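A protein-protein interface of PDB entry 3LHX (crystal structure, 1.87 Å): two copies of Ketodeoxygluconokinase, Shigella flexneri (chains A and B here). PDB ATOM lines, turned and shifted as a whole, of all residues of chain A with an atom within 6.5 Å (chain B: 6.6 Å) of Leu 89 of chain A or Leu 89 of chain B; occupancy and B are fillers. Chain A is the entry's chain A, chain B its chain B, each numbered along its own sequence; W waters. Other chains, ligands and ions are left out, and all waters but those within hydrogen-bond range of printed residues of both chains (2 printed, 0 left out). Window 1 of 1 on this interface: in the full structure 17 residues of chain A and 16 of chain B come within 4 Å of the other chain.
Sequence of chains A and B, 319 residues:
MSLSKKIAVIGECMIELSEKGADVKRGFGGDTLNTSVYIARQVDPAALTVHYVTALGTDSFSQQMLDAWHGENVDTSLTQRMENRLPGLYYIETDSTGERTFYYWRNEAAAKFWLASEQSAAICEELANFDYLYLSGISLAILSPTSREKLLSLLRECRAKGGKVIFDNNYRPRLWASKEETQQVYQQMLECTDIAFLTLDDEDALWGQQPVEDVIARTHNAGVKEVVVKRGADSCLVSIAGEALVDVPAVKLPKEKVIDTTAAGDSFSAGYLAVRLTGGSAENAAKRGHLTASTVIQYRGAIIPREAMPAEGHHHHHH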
ATOM      1  N   GLU A  12      11.397 -13.912 -12.317  1.00  0.00           N
ATOM      2  CA  GLU A  12      12.810 -13.713 -12.625  1.00  0.00           C
ATOM      3  C   GLU A  12      13.590 -15.016 -12.789  1.00  0.00           C
ATOM      4  O   GLU A  12      13.443 -15.951 -11.980  1.00  0.00           O
ATOM      5  CB  GLU A  12      13.479 -12.921 -11.501  1.00  0.00           C
ATOM      6  CG  GLU A  12      14.973 -12.690 -11.787  1.00  0.00           C
ATOM      7  CD  GLU A  12      15.639 -11.701 -10.846  1.00  0.00           C
ATOM      8  OE1 GLU A  12      15.025 -11.319  -9.812  1.00  0.00           O
ATOM      9  OE2 GLU A  12      16.806 -11.334 -11.134  1.00  0.00           O
ATOM     10  N   MET A  14      17.774 -15.902 -13.237  1.00  0.00           N
ATOM     11  CA  MET A  14      19.068 -15.307 -13.111  1.00  0.00           C
ATOM     12  C   MET A  14      20.125 -16.198 -13.781  1.00  0.00           C
ATOM     13  O   MET A  14      19.913 -17.393 -14.034  1.00  0.00           O
ATOM     14  CB  MET A  14      19.422 -15.124 -11.621  1.00  0.00           C
ATOM     15  CG  MET A  14      18.416 -14.220 -10.808  1.00  0.00           C
ATOM     16  SD  MET A  14      18.835 -14.263  -8.965  1.00  0.00           S
ATOM     17  CE  MET A  14      17.974 -16.008  -8.555  1.00  0.00           C
ATOM     18  N   ILE A  15      21.271 -15.596 -14.043  1.00  0.00           N
ATOM     19  CA  ILE A  15      22.492 -16.303 -14.353  1.00  0.00           C
ATOM     20  C   ILE A  15      22.964 -17.066 -13.108  1.00  0.00           C
ATOM     21  O   ILE A  15      23.068 -16.516 -12.016  1.00  0.00           O
ATOM     22  CB  ILE A  15      23.581 -15.262 -14.861  1.00  0.00           C
ATOM     23  CG1 ILE A  15      23.082 -14.507 -16.108  1.00  0.00           C
ATOM     24  CG2 ILE A  15      24.959 -15.939 -15.042  1.00  0.00           C
ATOM     25  CD1 ILE A  15      23.894 -13.218 -16.441  1.00  0.00           C
ATOM     26  N   GLU A  16      23.220 -18.353 -13.273  1.00  0.00           N
ATOM     27  CA  GLU A  16      23.598 -19.204 -12.178  1.00  0.00           C
ATOM     28  C   GLU A  16      25.029 -19.662 -12.361  1.00  0.00           C
ATOM     29  O   GLU A  16      25.363 -20.152 -13.428  1.00  0.00           O
ATOM     30  CB  GLU A  16      22.715 -20.462 -12.147  1.00  0.00           C
ATOM     31  CG  GLU A  16      23.088 -21.428 -11.040  1.00  0.00           C
ATOM     32  CD  GLU A  16      22.352 -22.759 -11.167  1.00  0.00           C
ATOM     33  OE1 GLU A  16      21.162 -22.795 -10.826  1.00  0.00           O
ATOM     34  OE2 GLU A  16      22.972 -23.753 -11.614  1.00  0.00           O
ATOM     35  N   LEU A  17      25.823 -19.525 -11.304  1.00  0.00           N
ATOM     36  CA  LEU A  17      27.164 -20.120 -11.198  1.00  0.00           C
ATOM     37  C   LEU A  17      27.186 -21.085 -10.026  1.00  0.00           C
ATOM     38  O   LEU A  17      26.710 -20.765  -8.917  1.00  0.00           O
ATOM     39  CB  LEU A  17      28.260 -19.040 -11.038  1.00  0.00           C
ATOM     40  CG  LEU A  17      28.443 -18.321 -12.374  1.00  0.00           C
ATOM     41  CD1 LEU A  17      28.326 -16.825 -12.317  1.00  0.00           C
ATOM     42  CD2 LEU A  17      29.703 -18.804 -13.117  1.00  0.00           C
ATOM     43  N   PHE A  61      24.437 -13.572 -22.429  1.00  0.00           N
ATOM     44  CA  PHE A  61      23.883 -14.371 -21.332  1.00  0.00           C
ATOM     45  C   PHE A  61      22.367 -14.407 -21.459  1.00  0.00           C
ATOM     46  O   PHE A  61      21.780 -15.470 -21.340  1.00  0.00           O
ATOM     47  CB  PHE A  61      24.218 -13.782 -19.967  1.00  0.00           C
ATOM     48  CG  PHE A  61      25.658 -13.830 -19.609  1.00  0.00           C
ATOM     49  CD1 PHE A  61      26.260 -15.022 -19.237  1.00  0.00           C
ATOM     50  CD2 PHE A  61      26.408 -12.657 -19.576  1.00  0.00           C
ATOM     51  CE1 PHE A  61      27.598 -15.057 -18.870  1.00  0.00           C
ATOM     52  CE2 PHE A  61      27.758 -12.677 -19.207  1.00  0.00           C
ATOM     53  CZ  PHE A  61      28.354 -13.874 -18.853  1.00  0.00           C
ATOM     54  N   PRO A  87      20.932  -9.508 -16.682  1.00  0.00           N
ATOM     55  CA  PRO A  87      20.204 -10.362 -15.750  1.00  0.00           C
ATOM     56  C   PRO A  87      20.810 -10.270 -14.370  1.00  0.00           C
ATOM     57  O   PRO A  87      21.997  -9.945 -14.227  1.00  0.00           O
ATOM     58  CB  PRO A  87      20.460 -11.789 -16.280  1.00  0.00           C
ATOM     59  CG  PRO A  87      20.792 -11.621 -17.697  1.00  0.00           C
ATOM     60  CD  PRO A  87      21.581 -10.306 -17.741  1.00  0.00           C
ATOM     61  N   GLY A  88      20.019 -10.615 -13.351  1.00  0.00           N
ATOM     62  CA  GLY A  88      20.616 -10.857 -12.039  1.00  0.00           C
ATOM     63  C   GLY A  88      21.527 -12.051 -12.131  1.00  0.00           C
ATOM     64  O   GLY A  88      21.441 -12.822 -13.091  1.00  0.00           O
ATOM     65  N   LEU A  89      22.374 -12.215 -11.122  1.00  0.00           N
ATOM     66  CA  LEU A  89      23.341 -13.279 -11.122  1.00  0.00           C
ATOM     67  C   LEU A  89      23.477 -13.821  -9.723  1.00  0.00           C
ATOM     68  O   LEU A  89      23.532 -13.039  -8.744  1.00  0.00           O
ATOM     69  CB  LEU A  89      24.711 -12.764 -11.634  1.00  0.00           C
ATOM     70  CG  LEU A  89      25.891 -13.729 -11.806  1.00  0.00           C
ATOM     71  CD1 LEU A  89      26.773 -13.325 -12.991  1.00  0.00           C
ATOM     72  CD2 LEU A  89      26.714 -13.813 -10.554  1.00  0.00           C
ATOM     73  N   TYR A  90      23.519 -15.153  -9.611  1.00  0.00           N
ATOM     74  CA  TYR A  90      23.757 -15.770  -8.313  1.00  0.00           C
ATOM     75  C   TYR A  90      24.844 -16.848  -8.336  1.00  0.00           C
ATOM     76  O   TYR A  90      25.182 -17.364  -9.393  1.00  0.00           O
ATOM     77  CB  TYR A  90      22.435 -16.249  -7.652  1.00  0.00           C
ATOM     78  CG  TYR A  90      21.797 -17.482  -8.240  1.00  0.00           C
ATOM     79  CD1 TYR A  90      21.851 -18.713  -7.565  1.00  0.00           C
ATOM     80  CD2 TYR A  90      21.157 -17.434  -9.458  1.00  0.00           C
ATOM     81  CE1 TYR A  90      21.254 -19.867  -8.094  1.00  0.00           C
ATOM     82  CE2 TYR A  90      20.554 -18.576 -10.008  1.00  0.00           C
ATOM     83  CZ  TYR A  90      20.608 -19.790  -9.319  1.00  0.00           C
ATOM     84  OH  TYR A  90      20.003 -20.914  -9.892  1.00  0.00           O
ATOM     85  N   TYR A  91      25.384 -17.158  -7.168  1.00  0.00           N
ATOM     86  CA  TYR A  91      26.523 -18.058  -7.059  1.00  0.00           C
ATOM     87  C   TYR A  91      26.325 -19.101  -5.975  1.00  0.00           C
ATOM     88  O   TYR A  91      26.171 -18.758  -4.799  1.00  0.00           O
ATOM     89  CB  TYR A  91      27.793 -17.271  -6.743  1.00  0.00           C
ATOM     90  CG  TYR A  91      29.070 -17.979  -7.130  1.00  0.00           C
ATOM     91  CD1 TYR A  91      29.594 -19.012  -6.342  1.00  0.00           C
ATOM     92  CD2 TYR A  91      29.767 -17.601  -8.281  1.00  0.00           C
ATOM     93  CE1 TYR A  91      30.785 -19.664  -6.704  1.00  0.00           C
ATOM     94  CE2 TYR A  91      30.960 -18.243  -8.645  1.00  0.00           C
ATOM     95  CZ  TYR A  91      31.456 -19.268  -7.857  1.00  0.00           C
ATOM     96  OH  TYR A  91      32.627 -19.900  -8.231  1.00  0.00           O
ATOM     97  N   TYR A 103      24.878 -16.812  -3.054  1.00  0.00           N
ATOM     98  CA  TYR A 103      25.306 -15.418  -3.082  1.00  0.00           C
ATOM     99  C   TYR A 103      24.634 -14.684  -4.225  1.00  0.00           C
ATOM    100  O   TYR A 103      24.545 -15.213  -5.325  1.00  0.00           O
ATOM    101  CB  TYR A 103      26.832 -15.322  -3.216  1.00  0.00           C
ATOM    102  CG  TYR A 103      27.622 -16.001  -2.118  1.00  0.00           C
ATOM    103  CD1 TYR A 103      27.940 -17.361  -2.197  1.00  0.00           C
ATOM    104  CD2 TYR A 103      28.090 -15.286  -1.033  1.00  0.00           C
ATOM    105  CE1 TYR A 103      28.681 -17.988  -1.217  1.00  0.00           C
ATOM    106  CE2 TYR A 103      28.860 -15.905  -0.029  1.00  0.00           C
ATOM    107  CZ  TYR A 103      29.145 -17.265  -0.125  1.00  0.00           C
ATOM    108  OH  TYR A 103      29.899 -17.892   0.865  1.00  0.00           O
ATOM    109  N   TYR A 104      24.153 -13.470  -3.969  1.00  0.00           N
ATOM    110  CA  TYR A 104      23.345 -12.764  -4.966  1.00  0.00           C
ATOM    111  C   TYR A 104      23.881 -11.396  -5.380  1.00  0.00           C
ATOM    112  O   TYR A 104      24.339 -10.607  -4.535  1.00  0.00           O
ATOM    113  CB  TYR A 104      21.899 -12.578  -4.471  1.00  0.00           C
ATOM    114  CG  TYR A 104      21.260 -13.889  -4.114  1.00  0.00           C
ATOM    115  CD1 TYR A 104      21.358 -14.382  -2.810  1.00  0.00           C
ATOM    116  CD2 TYR A 104      20.612 -14.673  -5.094  1.00  0.00           C
ATOM    117  CE1 TYR A 104      20.792 -15.629  -2.469  1.00  0.00           C
ATOM    118  CE2 TYR A 104      20.028 -15.928  -4.750  1.00  0.00           C
ATOM    119  CZ  TYR A 104      20.138 -16.372  -3.429  1.00  0.00           C
ATOM    120  OH  TYR A 104      19.595 -17.565  -3.059  1.00  0.00           O
ATOM    121  N   TRP A 105      23.692 -11.133  -6.667  1.00  0.00           N
ATOM    122  CA  TRP A 105      23.990  -9.885  -7.370  1.00  0.00           C
ATOM    123  C   TRP A 105      22.767  -9.624  -8.266  1.00  0.00           C
ATOM    124  O   TRP A 105      22.798  -9.679  -9.518  1.00  0.00           O
ATOM    125  CB  TRP A 105      25.337  -9.998  -8.165  1.00  0.00           C
ATOM    126  CG  TRP A 105      26.537 -10.053  -7.331  1.00  0.00           C
ATOM    127  CD1 TRP A 105      27.311  -8.987  -6.922  1.00  0.00           C
ATOM    128  CD2 TRP A 105      27.170 -11.238  -6.796  1.00  0.00           C
ATOM    129  NE1 TRP A 105      28.358  -9.449  -6.126  1.00  0.00           N
ATOM    130  CE2 TRP A 105      28.297 -10.819  -6.052  1.00  0.00           C
ATOM    131  CE3 TRP A 105      26.878 -12.612  -6.867  1.00  0.00           C
ATOM    132  CZ2 TRP A 105      29.127 -11.720  -5.360  1.00  0.00           C
ATOM    133  CZ3 TRP A 105      27.702 -13.509  -6.172  1.00  0.00           C
ATOM    134  CH2 TRP A 105      28.813 -13.057  -5.432  1.00  0.00           C
ATOM    135  N   ARG A 106      21.630  -9.360  -7.612  1.00  0.00           N
ATOM    136  CA  ARG A 106      20.380  -9.412  -8.304  1.00  0.00           C
ATOM    137  C   ARG A 106      19.647  -8.075  -8.247  1.00  0.00           C
ATOM    138  O   ARG A 106      18.613  -7.931  -8.856  1.00  0.00           O
ATOM    139  CB  ARG A 106      19.476 -10.552  -7.739  1.00  0.00           C
ATOM    140  CG  ARG A 106      18.954 -10.325  -6.304  1.00  0.00           C
ATOM    141  CD  ARG A 106      18.078 -11.510  -5.826  1.00  0.00           C
ATOM    142  NE  ARG A 106      16.960 -11.818  -6.728  1.00  0.00           N
ATOM    143  CZ  ARG A 106      16.303 -12.988  -6.739  1.00  0.00           C
ATOM    144  NH1 ARG A 106      16.638 -13.952  -5.880  1.00  0.00           N
ATOM    145  NH2 ARG A 106      15.308 -13.179  -7.579  1.00  0.00           N
ATOM    146  N   ALA A 109      18.793  -6.308 -11.657  1.00  0.00           N
ATOM    147  CA  ALA A 109      18.373  -7.145 -12.749  1.00  0.00           C
ATOM    148  C   ALA A 109      17.260  -6.523 -13.586  1.00  0.00           C
ATOM    149  O   ALA A 109      16.311  -5.896 -13.073  1.00  0.00           O
ATOM    150  CB  ALA A 109      17.925  -8.520 -12.180  1.00  0.00           C
ATOM    151  N   GLU B  12      39.228  -0.601  -5.908  1.00  0.00           N
ATOM    152  CA  GLU B  12      38.433  -1.829  -5.839  1.00  0.00           C
ATOM    153  C   GLU B  12      39.047  -3.035  -6.519  1.00  0.00           C
ATOM    154  O   GLU B  12      39.494  -2.926  -7.658  1.00  0.00           O
ATOM    155  CB  GLU B  12      37.106  -1.612  -6.563  1.00  0.00           C
ATOM    156  CG  GLU B  12      36.164  -2.820  -6.494  1.00  0.00           C
ATOM    157  CD  GLU B  12      34.740  -2.486  -6.909  1.00  0.00           C
ATOM    158  OE1 GLU B  12      34.480  -1.436  -7.537  1.00  0.00           O
ATOM    159  OE2 GLU B  12      33.868  -3.332  -6.629  1.00  0.00           O
ATOM    160  N   MET B  14      37.484  -6.916  -7.536  1.00  0.00           N
ATOM    161  CA  MET B  14      36.248  -7.664  -7.656  1.00  0.00           C
ATOM    162  C   MET B  14      36.520  -9.162  -7.706  1.00  0.00           C
ATOM    163  O   MET B  14      37.685  -9.595  -7.797  1.00  0.00           O
ATOM    164  CB  MET B  14      35.517  -7.223  -8.909  1.00  0.00           C
ATOM    165  CG  MET B  14      35.176  -5.722  -8.945  1.00  0.00           C
ATOM    166  SD  MET B  14      34.492  -5.167 -10.578  1.00  0.00           S
ATOM    167  CE  MET B  14      36.223  -4.981 -11.562  1.00  0.00           C
ATOM    168  N   ILE B  15      35.446  -9.938  -7.612  1.00  0.00           N
ATOM    169  CA  ILE B  15      35.440 -11.353  -7.936  1.00  0.00           C
ATOM    170  C   ILE B  15      35.476 -11.446  -9.455  1.00  0.00           C
ATOM    171  O   ILE B  15      34.731 -10.750 -10.164  1.00  0.00           O
ATOM    172  CB  ILE B  15      34.159 -12.056  -7.313  1.00  0.00           C
ATOM    173  CG1 ILE B  15      34.260 -12.049  -5.775  1.00  0.00           C
ATOM    174  CG2 ILE B  15      33.980 -13.468  -7.866  1.00  0.00           C
ATOM    175  CD1 ILE B  15      32.848 -12.095  -5.024  1.00  0.00           C
ATOM    176  N   GLU B  16      36.388 -12.258  -9.974  1.00  0.00           N
ATOM    177  CA  GLU B  16      36.529 -12.345 -11.425  1.00  0.00           C
ATOM    178  C   GLU B  16      36.095 -13.726 -11.967  1.00  0.00           C
ATOM    179  O   GLU B  16      36.570 -14.754 -11.483  1.00  0.00           O
ATOM    180  CB  GLU B  16      38.001 -12.120 -11.802  1.00  0.00           C
ATOM    181  CG  GLU B  16      38.305 -12.570 -13.239  1.00  0.00           C
ATOM    182  CD  GLU B  16      39.803 -12.650 -13.499  1.00  0.00           C
ATOM    183  OE1 GLU B  16      40.336 -11.537 -13.648  1.00  0.00           O
ATOM    184  OE2 GLU B  16      40.392 -13.786 -13.537  1.00  0.00           O
ATOM    185  N   LEU B  17      35.227 -13.736 -12.968  1.00  0.00           N
ATOM    186  CA  LEU B  17      34.890 -14.985 -13.659  1.00  0.00           C
ATOM    187  C   LEU B  17      35.309 -14.897 -15.120  1.00  0.00           C
ATOM    188  O   LEU B  17      35.037 -13.880 -15.767  1.00  0.00           O
ATOM    189  CB  LEU B  17      33.382 -15.285 -13.525  1.00  0.00           C
ATOM    190  CG  LEU B  17      32.920 -15.574 -12.086  1.00  0.00           C
ATOM    191  CD1 LEU B  17      31.456 -15.343 -11.942  1.00  0.00           C
ATOM    192  CD2 LEU B  17      33.285 -17.000 -11.646  1.00  0.00           C
ATOM    193  N   PHE B  61      34.558 -15.328  -0.259  1.00  0.00           N
ATOM    194  CA  PHE B  61      35.230 -14.732  -1.436  1.00  0.00           C
ATOM    195  C   PHE B  61      36.166 -13.612  -0.999  1.00  0.00           C
ATOM    196  O   PHE B  61      37.319 -13.539  -1.490  1.00  0.00           O
ATOM    197  CB  PHE B  61      34.247 -14.127  -2.462  1.00  0.00           C
ATOM    198  CG  PHE B  61      33.291 -15.110  -3.083  1.00  0.00           C
ATOM    199  CD1 PHE B  61      33.667 -15.900  -4.166  1.00  0.00           C
ATOM    200  CD2 PHE B  61      31.992 -15.227  -2.599  1.00  0.00           C
ATOM    201  CE1 PHE B  61      32.767 -16.817  -4.748  1.00  0.00           C
ATOM    202  CE2 PHE B  61      31.084 -16.119  -3.179  1.00  0.00           C
ATOM    203  CZ  PHE B  61      31.470 -16.920  -4.255  1.00  0.00           C
ATOM    204  N   PRO B  87      31.703  -8.453  -2.260  1.00  0.00           N
ATOM    205  CA  PRO B  87      32.496  -7.738  -3.277  1.00  0.00           C
ATOM    206  C   PRO B  87      31.660  -7.519  -4.526  1.00  0.00           C
ATOM    207  O   PRO B  87      30.602  -8.159  -4.676  1.00  0.00           O
ATOM    208  CB  PRO B  87      33.643  -8.723  -3.594  1.00  0.00           C
ATOM    209  CG  PRO B  87      33.751  -9.611  -2.372  1.00  0.00           C
ATOM    210  CD  PRO B  87      32.264  -9.802  -1.998  1.00  0.00           C
ATOM    211  N   GLY B  88      32.125  -6.656  -5.429  1.00  0.00           N
ATOM    212  CA  GLY B  88      31.537  -6.572  -6.778  1.00  0.00           C
ATOM    213  C   GLY B  88      32.014  -7.777  -7.556  1.00  0.00           C
ATOM    214  O   GLY B  88      32.962  -8.445  -7.118  1.00  0.00           O
ATOM    215  N   LEU B  89      31.379  -8.063  -8.683  1.00  0.00           N
ATOM    216  CA  LEU B  89      31.735  -9.250  -9.479  1.00  0.00           C
ATOM    217  C   LEU B  89      31.749  -8.881 -10.939  1.00  0.00           C
ATOM    218  O   LEU B  89      30.899  -8.120 -11.394  1.00  0.00           O
ATOM    219  CB  LEU B  89      30.705 -10.387  -9.194  1.00  0.00           C
ATOM    220  CG  LEU B  89      30.800 -11.735  -9.912  1.00  0.00           C
ATOM    221  CD1 LEU B  89      30.145 -12.850  -9.063  1.00  0.00           C
ATOM    222  CD2 LEU B  89      30.161 -11.653 -11.300  1.00  0.00           C
ATOM    223  N   TYR B  90      32.707  -9.430 -11.693  1.00  0.00           N
ATOM    224  CA  TYR B  90      32.746  -9.185 -13.130  1.00  0.00           C
ATOM    225  C   TYR B  90      33.013 -10.487 -13.866  1.00  0.00           C
ATOM    226  O   TYR B  90      33.552 -11.415 -13.308  1.00  0.00           O
ATOM    227  CB  TYR B  90      33.784  -8.094 -13.523  1.00  0.00           C
ATOM    228  CG  TYR B  90      35.261  -8.420 -13.413  1.00  0.00           C
ATOM    229  CD1 TYR B  90      36.059  -8.498 -14.576  1.00  0.00           C
ATOM    230  CD2 TYR B  90      35.891  -8.581 -12.202  1.00  0.00           C
ATOM    231  CE1 TYR B  90      37.436  -8.757 -14.517  1.00  0.00           C
ATOM    232  CE2 TYR B  90      37.293  -8.836 -12.124  1.00  0.00           C
ATOM    233  CZ  TYR B  90      38.056  -8.938 -13.296  1.00  0.00           C
ATOM    234  OH  TYR B  90      39.440  -9.216 -13.255  1.00  0.00           O
ATOM    235  N   TYR B  91      32.623 -10.524 -15.124  1.00  0.00           N
ATOM    236  CA  TYR B  91      32.705 -11.754 -15.887  1.00  0.00           C
ATOM    237  C   TYR B  91      33.393 -11.452 -17.200  1.00  0.00           C
ATOM    238  O   TYR B  91      32.990 -10.535 -17.883  1.00  0.00           O
ATOM    239  CB  TYR B  91      31.290 -12.257 -16.177  1.00  0.00           C
ATOM    240  CG  TYR B  91      31.231 -13.736 -16.459  1.00  0.00           C
ATOM    241  CD1 TYR B  91      31.664 -14.255 -17.693  1.00  0.00           C
ATOM    242  CD2 TYR B  91      30.748 -14.630 -15.487  1.00  0.00           C
ATOM    243  CE1 TYR B  91      31.612 -15.649 -17.946  1.00  0.00           C
ATOM    244  CE2 TYR B  91      30.692 -16.013 -15.727  1.00  0.00           C
ATOM    245  CZ  TYR B  91      31.130 -16.517 -16.953  1.00  0.00           C
ATOM    246  OH  TYR B  91      31.070 -17.879 -17.191  1.00  0.00           O
ATOM    247  N   TYR B 103      31.430  -7.854 -18.300  1.00  0.00           N
ATOM    248  CA  TYR B 103      30.091  -7.675 -17.731  1.00  0.00           C
ATOM    249  C   TYR B 103      30.277  -7.447 -16.231  1.00  0.00           C
ATOM    250  O   TYR B 103      31.046  -8.126 -15.613  1.00  0.00           O
ATOM    251  CB  TYR B 103      29.259  -8.935 -17.964  1.00  0.00           C
ATOM    252  CG  TYR B 103      29.018  -9.274 -19.442  1.00  0.00           C
ATOM    253  CD1 TYR B 103      29.864 -10.165 -20.137  1.00  0.00           C
ATOM    254  CD2 TYR B 103      27.932  -8.722 -20.134  1.00  0.00           C
ATOM    255  CE1 TYR B 103      29.623 -10.480 -21.481  1.00  0.00           C
ATOM    256  CE2 TYR B 103      27.680  -9.036 -21.481  1.00  0.00           C
ATOM    257  CZ  TYR B 103      28.530  -9.914 -22.145  1.00  0.00           C
ATOM    258  OH  TYR B 103      28.258 -10.221 -23.468  1.00  0.00           O
ATOM    259  N   TYR B 104      29.577  -6.469 -15.668  1.00  0.00           N
ATOM    260  CA  TYR B 104      29.823  -6.083 -14.296  1.00  0.00           C
ATOM    261  C   TYR B 104      28.547  -6.206 -13.439  1.00  0.00           C
ATOM    262  O   TYR B 104      27.467  -5.870 -13.888  1.00  0.00           O
ATOM    263  CB  TYR B 104      30.411  -4.643 -14.244  1.00  0.00           C
ATOM    264  CG  TYR B 104      31.826  -4.594 -14.827  1.00  0.00           C
ATOM    265  CD1 TYR B 104      32.040  -4.229 -16.149  1.00  0.00           C
ATOM    266  CD2 TYR B 104      32.939  -5.004 -14.065  1.00  0.00           C
ATOM    267  CE1 TYR B 104      33.343  -4.225 -16.691  1.00  0.00           C
ATOM    268  CE2 TYR B 104      34.231  -5.005 -14.599  1.00  0.00           C
ATOM    269  CZ  TYR B 104      34.420  -4.621 -15.909  1.00  0.00           C
ATOM    270  OH  TYR B 104      35.719  -4.631 -16.430  1.00  0.00           O
ATOM    271  N   TRP B 105      28.738  -6.729 -12.235  1.00  0.00           N
ATOM    272  CA  TRP B 105      27.726  -6.693 -11.160  1.00  0.00           C
ATOM    273  C   TRP B 105      28.417  -6.000  -9.998  1.00  0.00           C
ATOM    274  O   TRP B 105      28.789  -6.627  -9.018  1.00  0.00           O
ATOM    275  CB  TRP B 105      27.297  -8.134 -10.799  1.00  0.00           C
ATOM    276  CG  TRP B 105      26.415  -8.671 -11.832  1.00  0.00           C
ATOM    277  CD1 TRP B 105      25.029  -8.592 -11.872  1.00  0.00           C
ATOM    278  CD2 TRP B 105      26.809  -9.359 -13.039  1.00  0.00           C
ATOM    279  NE1 TRP B 105      24.561  -9.187 -13.013  1.00  0.00           N
ATOM    280  CE2 TRP B 105      25.617  -9.665 -13.750  1.00  0.00           C
ATOM    281  CE3 TRP B 105      28.049  -9.726 -13.596  1.00  0.00           C
ATOM    282  CZ2 TRP B 105      25.625 -10.329 -15.004  1.00  0.00           C
ATOM    283  CZ3 TRP B 105      28.058 -10.417 -14.852  1.00  0.00           C
ATOM    284  CH2 TRP B 105      26.852 -10.706 -15.522  1.00  0.00           C
ATOM    285  N   ARG B 106      28.657  -4.693 -10.128  1.00  0.00           N
ATOM    286  CA  ARG B 106      29.556  -4.030  -9.159  1.00  0.00           C
ATOM    287  C   ARG B 106      28.923  -2.831  -8.426  1.00  0.00           C
ATOM    288  O   ARG B 106      29.580  -2.216  -7.585  1.00  0.00           O
ATOM    289  CB  ARG B 106      30.880  -3.570  -9.827  1.00  0.00           C
ATOM    290  CG  ARG B 106      30.690  -2.410 -10.809  1.00  0.00           C
ATOM    291  CD  ARG B 106      32.003  -1.967 -11.557  1.00  0.00           C
ATOM    292  NE  ARG B 106      33.097  -1.649 -10.660  1.00  0.00           N
ATOM    293  CZ  ARG B 106      34.378  -1.570 -11.066  1.00  0.00           C
ATOM    294  NH1 ARG B 106      34.673  -1.765 -12.343  1.00  0.00           N
ATOM    295  NH2 ARG B 106      35.344  -1.323 -10.208  1.00  0.00           N
ATOM    296  N   ALA B 109      28.997  -2.999  -4.590  1.00  0.00           N
ATOM    297  CA  ALA B 109      30.209  -3.423  -3.926  1.00  0.00           C
ATOM    298  C   ALA B 109      30.484  -2.674  -2.610  1.00  0.00           C
ATOM    299  O   ALA B 109      30.392  -1.439  -2.549  1.00  0.00           O
ATOM    300  CB  ALA B 109      31.467  -3.285  -4.907  1.00  0.00           C
HETATM  301  O   HOH W   1      22.045  -6.976 -13.313  1.00  0.00           O
HETATM  302  O   HOH W   2      28.071  -6.678  -4.287  1.00  0.00           O
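Leu 17 of chain A touches its own counterpart, Leu 17 of chain B. Phe 61 of chain A touches Tyr 103 of chain B, and with the chains exchanged Tyr 103 of chain A touches Phe 61 of chain B. Leu 89 of chain B touches its own counterpart, Leu 89 of chain A. Leu 89 of chain A touches Trp 105 of chain B, and with the chains exchanged Trp 105 of chain A touches Leu 89 of chain B. Positions printed for both chains: 12, 14, 15, 16, 17, 61, 87, 88, 89, 90, 91, 103, 104, 105, 106 and 109.
The backbone carbonyl oxygen of Pro 87 of chain A is in hydrogen-bond range of the indole nitrogen of Trp 105 of chain B, at 2.9 Å. O of Pro 87 of chain B is in hydrogen-bond range of NE1 of Trp 105 of chain A, 3.0 Å away.
Water W2 lies within hydrogen-bond range of O of Pro 87 of chain B and NE1 of Trp 105 of chain A. Water W1 bridges the backbone carbonyl oxygen (O) of Pro 87 of chain A (3.1 Å) and the indole nitrogen (NE1) of Trp 105 of chain B (3.4 Å).
Of chain B, only Leu 89 (3.9 Å) and Trp 105 (3.6 Å) come within 4 Å of Leu 89 of chain A. Of chain A, only Leu 89 and Trp 105 come within 4 Å of Leu 89 of chain B. Of the printed residues of chain A, Leu 17 of chain B touches Leu 17 (3.5 Å) and Tyr 91 (3.99 Å). Printed residues of chain A within 4 Å of Tyr 103 of chain B: Phe 61 (3.4 Å). The nearest printed residue of chain B that does not touch Tyr 103 of chain A is Pro 87 of chain B (7.0 Å).
Printed residues of chain B that touch a printed residue of chain A: Ile 15, Leu 17, Phe 61, Pro 87, Leu 89, Tyr 91, Tyr 103 and Trp 105. Hydrophobic or aromatic side chains of chain B that line the printed part of chain A: Ile 15, Leu 17, Phe 61, Leu 89, Tyr 91, Tyr 103 and Trp 105. Among the printed residues, 15 pairs touch across the chains.
Leu 17 of chain A touches Leu 17 of chain B. Phe 61 of chain A touches Tyr 91 of chain B. Tyr 103 of chain B touches Phe 61 of chain A (CD1 to CE2, 3.4 Å). Leu 89 of chain A touches Leu 89 of chain B. Leu 89 of chain A touches Trp 105 of chain B (CD1 to CH2, 3.6 Å). Leu 17 of chain B touches Tyr 91 of chain A. CZ of Phe 61 of chain B touches CD1 of Tyr 91 of chain A, at 3.5 Å. Ile 15 of chain B touches Trp 105 of chain A. Trp 105 of chain A touches Leu 89 of chain B (CZ3 to CD1, 3.8 Å). Trp 105 of chain B touches Trp 105 of chain A.
N of Ile 15 of chain B is in hydrogen-bond range of O of Gly 88 of chain B. O of Leu 89 of chain A is in hydrogen-bond range of N of Trp 105 of chain A. The backbone carbonyl oxygen (O) of Tyr 103 of chain B sits at hydrogen-bond distance from the backbone NH (N) of Tyr 91 of chain B, 2.9 Å away. The backbone NH (N) of Leu 17 of chain B lies within hydrogen-bond range of the backbone carbonyl oxygen (O) of Tyr 90 of chain B (2.9 Å). O of Gly 88 of chain A lies within hydrogen-bond range of N of Ile 15 of chain A (2.9 Å).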
